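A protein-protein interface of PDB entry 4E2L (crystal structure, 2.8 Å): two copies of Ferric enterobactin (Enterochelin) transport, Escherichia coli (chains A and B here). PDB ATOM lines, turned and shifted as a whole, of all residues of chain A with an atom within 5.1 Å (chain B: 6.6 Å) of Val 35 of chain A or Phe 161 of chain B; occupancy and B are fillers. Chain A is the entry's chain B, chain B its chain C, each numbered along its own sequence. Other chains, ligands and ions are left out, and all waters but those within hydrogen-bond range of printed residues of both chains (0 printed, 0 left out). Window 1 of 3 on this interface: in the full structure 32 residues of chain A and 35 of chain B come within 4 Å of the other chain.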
ATOM      1  N   THR A  31      -6.205  23.158   4.803  1.00  0.00           N
ATOM      2  CA  THR A  31      -7.274  22.614   3.975  1.00  0.00           C
ATOM      3  C   THR A  31      -7.680  21.216   4.438  1.00  0.00           C
ATOM      4  O   THR A  31      -8.868  20.876   4.439  1.00  0.00           O
ATOM      5  CB  THR A  31      -6.898  22.608   2.477  1.00  0.00           C
ATOM      6  OG1 THR A  31      -7.207  23.885   1.913  1.00  0.00           O
ATOM      7  CG2 THR A  31      -7.692  21.563   1.732  1.00  0.00           C
ATOM      8  N   LYS A  32      -6.699  20.411   4.836  1.00  0.00           N
ATOM      9  CA  LYS A  32      -7.000  19.120   5.441  1.00  0.00           C
ATOM     10  C   LYS A  32      -7.965  19.304   6.623  1.00  0.00           C
ATOM     11  O   LYS A  32      -8.896  18.513   6.813  1.00  0.00           O
ATOM     12  CB  LYS A  32      -5.716  18.408   5.880  1.00  0.00           C
ATOM     13  N   LEU A  33      -7.756  20.373   7.389  1.00  0.00           N
ATOM     14  CA  LEU A  33      -8.511  20.624   8.614  1.00  0.00           C
ATOM     15  C   LEU A  33      -9.851  21.311   8.388  1.00  0.00           C
ATOM     16  O   LEU A  33     -10.768  21.177   9.199  1.00  0.00           O
ATOM     17  CB  LEU A  33      -7.694  21.497   9.562  1.00  0.00           C
ATOM     18  CG  LEU A  33      -6.435  20.901  10.172  1.00  0.00           C
ATOM     19  CD1 LEU A  33      -5.890  21.910  11.163  1.00  0.00           C
ATOM     20  CD2 LEU A  33      -6.728  19.554  10.837  1.00  0.00           C
ATOM     21  N   ARG A  34      -9.939  22.093   7.318  1.00  0.00           N
ATOM     22  CA  ARG A  34     -11.164  22.809   7.004  1.00  0.00           C
ATOM     23  C   ARG A  34     -12.229  21.753   6.737  1.00  0.00           C
ATOM     24  O   ARG A  34     -13.378  21.875   7.170  1.00  0.00           O
ATOM     25  CB  ARG A  34     -10.953  23.707   5.781  1.00  0.00           C
ATOM     26  CG  ARG A  34     -11.985  24.823   5.605  1.00  0.00           C
ATOM     27  CD  ARG A  34     -11.579  25.778   4.471  1.00  0.00           C
ATOM     28  NE  ARG A  34     -10.234  26.321   4.674  1.00  0.00           N
ATOM     29  CZ  ARG A  34      -9.336  26.500   3.707  1.00  0.00           C
ATOM     30  NH1 ARG A  34      -9.634  26.185   2.450  1.00  0.00           N
ATOM     31  NH2 ARG A  34      -8.136  26.994   3.999  1.00  0.00           N
ATOM     32  N   VAL A  35     -11.815  20.704   6.035  1.00  0.00           N
ATOM     33  CA  VAL A  35     -12.658  19.551   5.775  1.00  0.00           C
ATOM     34  C   VAL A  35     -13.230  18.977   7.066  1.00  0.00           C
ATOM     35  O   VAL A  35     -14.394  18.595   7.110  1.00  0.00           O
ATOM     36  CB  VAL A  35     -11.870  18.463   5.033  1.00  0.00           C
ATOM     37  CG1 VAL A  35     -12.692  17.200   4.920  1.00  0.00           C
ATOM     38  CG2 VAL A  35     -11.456  18.965   3.657  1.00  0.00           C
ATOM     39  N   LEU A  36     -12.411  18.910   8.109  1.00  0.00           N
ATOM     40  CA  LEU A  36     -12.838  18.408   9.411  1.00  0.00           C
ATOM     41  C   LEU A  36     -13.507  19.512  10.214  1.00  0.00           C
ATOM     42  O   LEU A  36     -13.464  19.511  11.446  1.00  0.00           O
ATOM     43  CB  LEU A  36     -11.641  17.861  10.192  1.00  0.00           C
ATOM     44  CG  LEU A  36     -11.079  16.476   9.839  1.00  0.00           C
ATOM     45  CD1 LEU A  36     -11.153  16.177   8.357  1.00  0.00           C
ATOM     46  CD2 LEU A  36      -9.641  16.329  10.323  1.00  0.00           C
ATOM     47  N   ASP A  37     -14.120  20.448   9.492  1.00  0.00           N
ATOM     48  CA  ASP A  37     -14.725  21.670  10.055  1.00  0.00           C
ATOM     49  C   ASP A  37     -13.866  22.399  11.124  1.00  0.00           C
ATOM     50  O   ASP A  37     -14.344  22.814  12.193  1.00  0.00           O
ATOM     51  CB  ASP A  37     -16.202  21.446  10.470  1.00  0.00           C
ATOM     52  CG  ASP A  37     -16.391  21.320  11.981  1.00  0.00           C
ATOM     53  OD1 ASP A  37     -15.570  20.636  12.653  1.00  0.00           O
ATOM     54  OD2 ASP A  37     -17.372  21.921  12.489  1.00  0.00           O
ATOM     55  N   GLU B 156      -4.722  23.681  -7.038  1.00  0.00           N
ATOM     56  CA  GLU B 156      -4.347  22.530  -6.236  1.00  0.00           C
ATOM     57  C   GLU B 156      -5.165  22.489  -4.948  1.00  0.00           C
ATOM     58  O   GLU B 156      -5.749  21.469  -4.616  1.00  0.00           O
ATOM     59  CB  GLU B 156      -2.847  22.543  -5.944  1.00  0.00           C
ATOM     60  CG  GLU B 156      -2.391  21.473  -4.968  1.00  0.00           C
ATOM     61  CD  GLU B 156      -0.867  21.334  -4.876  1.00  0.00           C
ATOM     62  OE1 GLU B 156      -0.186  22.346  -4.569  1.00  0.00           O
ATOM     63  OE2 GLU B 156      -0.352  20.207  -5.104  1.00  0.00           O
ATOM     64  N   ILE B 157      -5.221  23.601  -4.231  1.00  0.00           N
ATOM     65  CA  ILE B 157      -5.974  23.664  -2.978  1.00  0.00           C
ATOM     66  C   ILE B 157      -7.458  23.394  -3.211  1.00  0.00           C
ATOM     67  O   ILE B 157      -8.156  22.835  -2.354  1.00  0.00           O
ATOM     68  CB  ILE B 157      -5.763  25.024  -2.262  1.00  0.00           C
ATOM     69  CG1 ILE B 157      -4.403  25.037  -1.577  1.00  0.00           C
ATOM     70  CG2 ILE B 157      -6.857  25.302  -1.241  1.00  0.00           C
ATOM     71  CD1 ILE B 157      -4.259  23.982  -0.548  1.00  0.00           C
ATOM     72  N   LYS B 158      -7.936  23.793  -4.381  1.00  0.00           N
ATOM     73  CA  LYS B 158      -9.328  23.580  -4.729  1.00  0.00           C
ATOM     74  C   LYS B 158      -9.549  22.106  -5.032  1.00  0.00           C
ATOM     75  O   LYS B 158     -10.404  21.461  -4.425  1.00  0.00           O
ATOM     76  CB  LYS B 158      -9.727  24.453  -5.915  1.00  0.00           C
ATOM     77  CG  LYS B 158     -10.994  25.251  -5.680  1.00  0.00           C
ATOM     78  CD  LYS B 158     -12.236  24.424  -5.972  1.00  0.00           C
ATOM     79  CE  LYS B 158     -13.473  25.145  -5.497  1.00  0.00           C
ATOM     80  NZ  LYS B 158     -14.700  24.537  -6.065  1.00  0.00           N
ATOM     81  N   THR B 159      -8.765  21.565  -5.958  1.00  0.00           N
ATOM     82  CA  THR B 159      -8.846  20.143  -6.247  1.00  0.00           C
ATOM     83  C   THR B 159      -8.780  19.336  -4.958  1.00  0.00           C
ATOM     84  O   THR B 159      -9.667  18.542  -4.690  1.00  0.00           O
ATOM     85  CB  THR B 159      -7.747  19.678  -7.207  1.00  0.00           C
ATOM     86  OG1 THR B 159      -7.919  20.321  -8.473  1.00  0.00           O
ATOM     87  CG2 THR B 159      -7.823  18.176  -7.406  1.00  0.00           C
ATOM     88  N   GLN B 160      -7.742  19.541  -4.154  1.00  0.00           N
ATOM     89  CA  GLN B 160      -7.597  18.765  -2.928  1.00  0.00           C
ATOM     90  C   GLN B 160      -8.824  18.863  -2.031  1.00  0.00           C
ATOM     91  O   GLN B 160      -9.363  17.849  -1.609  1.00  0.00           O
ATOM     92  CB  GLN B 160      -6.368  19.178  -2.134  1.00  0.00           C
ATOM     93  CG  GLN B 160      -6.483  18.763  -0.677  1.00  0.00           C
ATOM     94  CD  GLN B 160      -5.378  19.321   0.191  1.00  0.00           C
ATOM     95  OE1 GLN B 160      -5.612  19.698   1.343  1.00  0.00           O
ATOM     96  NE2 GLN B 160      -4.159  19.368  -0.350  1.00  0.00           N
ATOM     97  N   PHE B 161      -9.273  20.074  -1.739  1.00  0.00           N
ATOM     98  CA  PHE B 161     -10.415  20.250  -0.855  1.00  0.00           C
ATOM     99  C   PHE B 161     -11.663  19.511  -1.347  1.00  0.00           C
ATOM    100  O   PHE B 161     -12.336  18.814  -0.583  1.00  0.00           O
ATOM    101  CB  PHE B 161     -10.735  21.728  -0.679  1.00  0.00           C
ATOM    102  CG  PHE B 161     -11.977  21.971   0.094  1.00  0.00           C
ATOM    103  CD1 PHE B 161     -11.935  22.070   1.471  1.00  0.00           C
ATOM    104  CD2 PHE B 161     -13.199  22.065  -0.552  1.00  0.00           C
ATOM    105  CE1 PHE B 161     -13.084  22.274   2.198  1.00  0.00           C
ATOM    106  CE2 PHE B 161     -14.355  22.267   0.165  1.00  0.00           C
ATOM    107  CZ  PHE B 161     -14.300  22.374   1.545  1.00  0.00           C
ATOM    108  N   GLU B 162     -11.978  19.673  -2.627  1.00  0.00           N
ATOM    109  CA  GLU B 162     -13.112  18.977  -3.235  1.00  0.00           C
ATOM    110  C   GLU B 162     -13.002  17.448  -3.190  1.00  0.00           C
ATOM    111  O   GLU B 162     -14.005  16.748  -3.102  1.00  0.00           O
ATOM    112  CB  GLU B 162     -13.294  19.436  -4.685  1.00  0.00           C
ATOM    113  CG  GLU B 162     -13.783  20.864  -4.830  1.00  0.00           C
ATOM    114  CD  GLU B 162     -15.100  21.103  -4.114  1.00  0.00           C
ATOM    115  OE1 GLU B 162     -15.620  20.161  -3.474  1.00  0.00           O
ATOM    116  OE2 GLU B 162     -15.622  22.234  -4.189  1.00  0.00           O
ATOM    117  N   LYS B 163     -11.777  16.947  -3.270  1.00  0.00           N
ATOM    118  CA  LYS B 163     -11.517  15.522  -3.291  1.00  0.00           C
ATOM    119  C   LYS B 163     -11.669  14.958  -1.885  1.00  0.00           C
ATOM    120  O   LYS B 163     -12.243  13.884  -1.677  1.00  0.00           O
ATOM    121  CB  LYS B 163     -10.107  15.261  -3.835  1.00  0.00           C
ATOM    122  CG  LYS B 163      -9.646  13.821  -3.765  1.00  0.00           C
ATOM    123  N   GLU B 164     -11.164  15.686  -0.904  1.00  0.00           N
ATOM    124  CA  GLU B 164     -11.238  15.187   0.456  1.00  0.00           C
ATOM    125  C   GLU B 164     -12.643  15.372   1.021  1.00  0.00           C
ATOM    126  O   GLU B 164     -13.040  14.681   1.945  1.00  0.00           O
ATOM    127  CB  GLU B 164     -10.172  15.844   1.345  1.00  0.00           C
ATOM    128  N   LYS B 165     -13.405  16.298   0.463  1.00  0.00           N
ATOM    129  CA  LYS B 165     -14.747  16.517   0.973  1.00  0.00           C
ATOM    130  C   LYS B 165     -15.673  15.426   0.469  1.00  0.00           C
ATOM    131  O   LYS B 165     -16.590  15.027   1.172  1.00  0.00           O
ATOM    132  CB  LYS B 165     -15.282  17.886   0.563  1.00  0.00           C
ATOM    133  CG  LYS B 165     -15.681  18.774   1.724  1.00  0.00           C
ATOM    134  CD  LYS B 165     -16.805  18.167   2.518  1.00  0.00           C
ATOM    135  CE  LYS B 165     -17.155  19.040   3.710  1.00  0.00           C
ATOM    136  NZ  LYS B 165     -18.254  18.452   4.533  1.00  0.00           N
ATOM    137  N   LEU B 166     -15.427  14.956  -0.753  1.00  0.00           N
ATOM    138  CA  LEU B 166     -16.190  13.854  -1.339  1.00  0.00           C
ATOM    139  C   LEU B 166     -15.911  12.572  -0.564  1.00  0.00           C
ATOM    140  O   LEU B 166     -16.830  11.944  -0.036  1.00  0.00           O
ATOM    141  CB  LEU B 166     -15.800  13.651  -2.803  1.00  0.00           C
ATOM    142  CG  LEU B 166     -16.753  12.810  -3.644  1.00  0.00           C
ATOM    143  CD1 LEU B 166     -18.085  13.495  -3.654  1.00  0.00           C
ATOM    144  CD2 LEU B 166     -16.236  12.622  -5.065  1.00  0.00           C
ATOM    145  N   GLN B 168     -15.085  12.108   2.232  1.00  0.00           N
ATOM    146  CA  GLN B 168     -15.718  12.147   3.551  1.00  0.00           C
ATOM    147  C   GLN B 168     -17.262  12.112   3.482  1.00  0.00           C
ATOM    148  O   GLN B 168     -17.915  11.687   4.432  1.00  0.00           O
ATOM    149  CB  GLN B 168     -15.209  13.353   4.365  1.00  0.00           C
ATOM    150  CG  GLN B 168     -16.286  14.355   4.774  1.00  0.00           C
ATOM    151  CD  GLN B 168     -15.952  15.089   6.070  1.00  0.00           C
ATOM    152  OE1 GLN B 168     -15.192  14.587   6.900  1.00  0.00           O
ATOM    153  NE2 GLN B 168     -16.525  16.279   6.249  1.00  0.00           N
ATOM    154  N   ARG B 241     -20.477  15.161  -8.307  1.00  0.00           N
ATOM    155  CA  ARG B 241     -19.356  15.651  -7.523  1.00  0.00           C
ATOM    156  C   ARG B 241     -18.103  14.918  -7.986  1.00  0.00           C
ATOM    157  O   ARG B 241     -17.087  15.543  -8.262  1.00  0.00           O
ATOM    158  CB  ARG B 241     -19.608  15.528  -6.023  1.00  0.00           C
ATOM    159  CG  ARG B 241     -20.533  16.620  -5.489  1.00  0.00           C
ATOM    160  CD  ARG B 241     -20.836  16.484  -4.001  1.00  0.00           C
ATOM    161  NE  ARG B 241     -19.653  16.682  -3.172  1.00  0.00           N
ATOM    162  CZ  ARG B 241     -19.660  16.674  -1.841  1.00  0.00           C
ATOM    163  NH1 ARG B 241     -18.535  16.861  -1.159  1.00  0.00           N
ATOM    164  NH2 ARG B 241     -20.794  16.479  -1.189  1.00  0.00           N
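Printed residues of chain B within 4 Å of Lys 32 of chain A: Gln 160. Leu 33 of chain A touches none of the printed residues of chain B. Printed residues of chain A within 4 Å of Ile 157 of chain B: Thr 31 (3.5 Å). Of the printed residues of chain A, Gln 160 of chain B touches Thr 31 and Lys 32. Printed residues of chain A within 4 Å of Glu 164 of chain B: Val 35. Of the printed residues of chain A, Gln 168 of chain B touches Val 35. The nearest residue of chain A that does not touch Phe 161 of chain B is Arg 34 of chain A (4.4 Å). The nearest printed residue of chain A that does not touch Gln 168 of chain B is Leu 36 of chain A (4.6 Å).
NH1 of Arg 34 of chain A lies within hydrogen-bond range of OG1 of Thr 31 of chain A, 3.4 Å away. The side-chain amino group (NZ) of Lys 165 of chain B lies close to the side-chain amide nitrogen (NE2) of Gln 168 of chain B (3.3 Å).
No position is printed for both chains. Of the 7 pairs that touch across the chains among the printed residues, none has its exchanged pair printed and touching as well.
Thr 31 of chain A touches Ile 157 of chain B. Gln 160 of chain B touches Thr 31 of chain A. Phe 161 of chain B touches Thr 31 of chain A (CB to CG2, 3.9 Å). Gln 160 of chain B touches Lys 32 of chain A (OE1 to N, 3.7 Å). Val 35 of chain A touches Phe 161 of chain B (CG2 to CD1, 3.8 Å). Glu 164 of chain B touches Val 35 of chain A.
The backbone carbonyl oxygen (O) of Val 35 of chain A lies within hydrogen-bond range of the side-chain amide nitrogen (NE2) of Gln 168 of chain B (3.3 Å).
Of the 13 printed residues of chain B, 5 touch a printed residue of chain A. Along chain B the printed residues that touch a printed residue of chain A span positions 157 to 168. Printed residues of chain A that touch a printed residue of chain B: Thr 31, Lys 32 and Val 35. Hydrophobic or aromatic side chains of chain A within 4 Å of the printed part of chain B: Val 35. Among the printed residues, 7 pairs touch across the chains.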
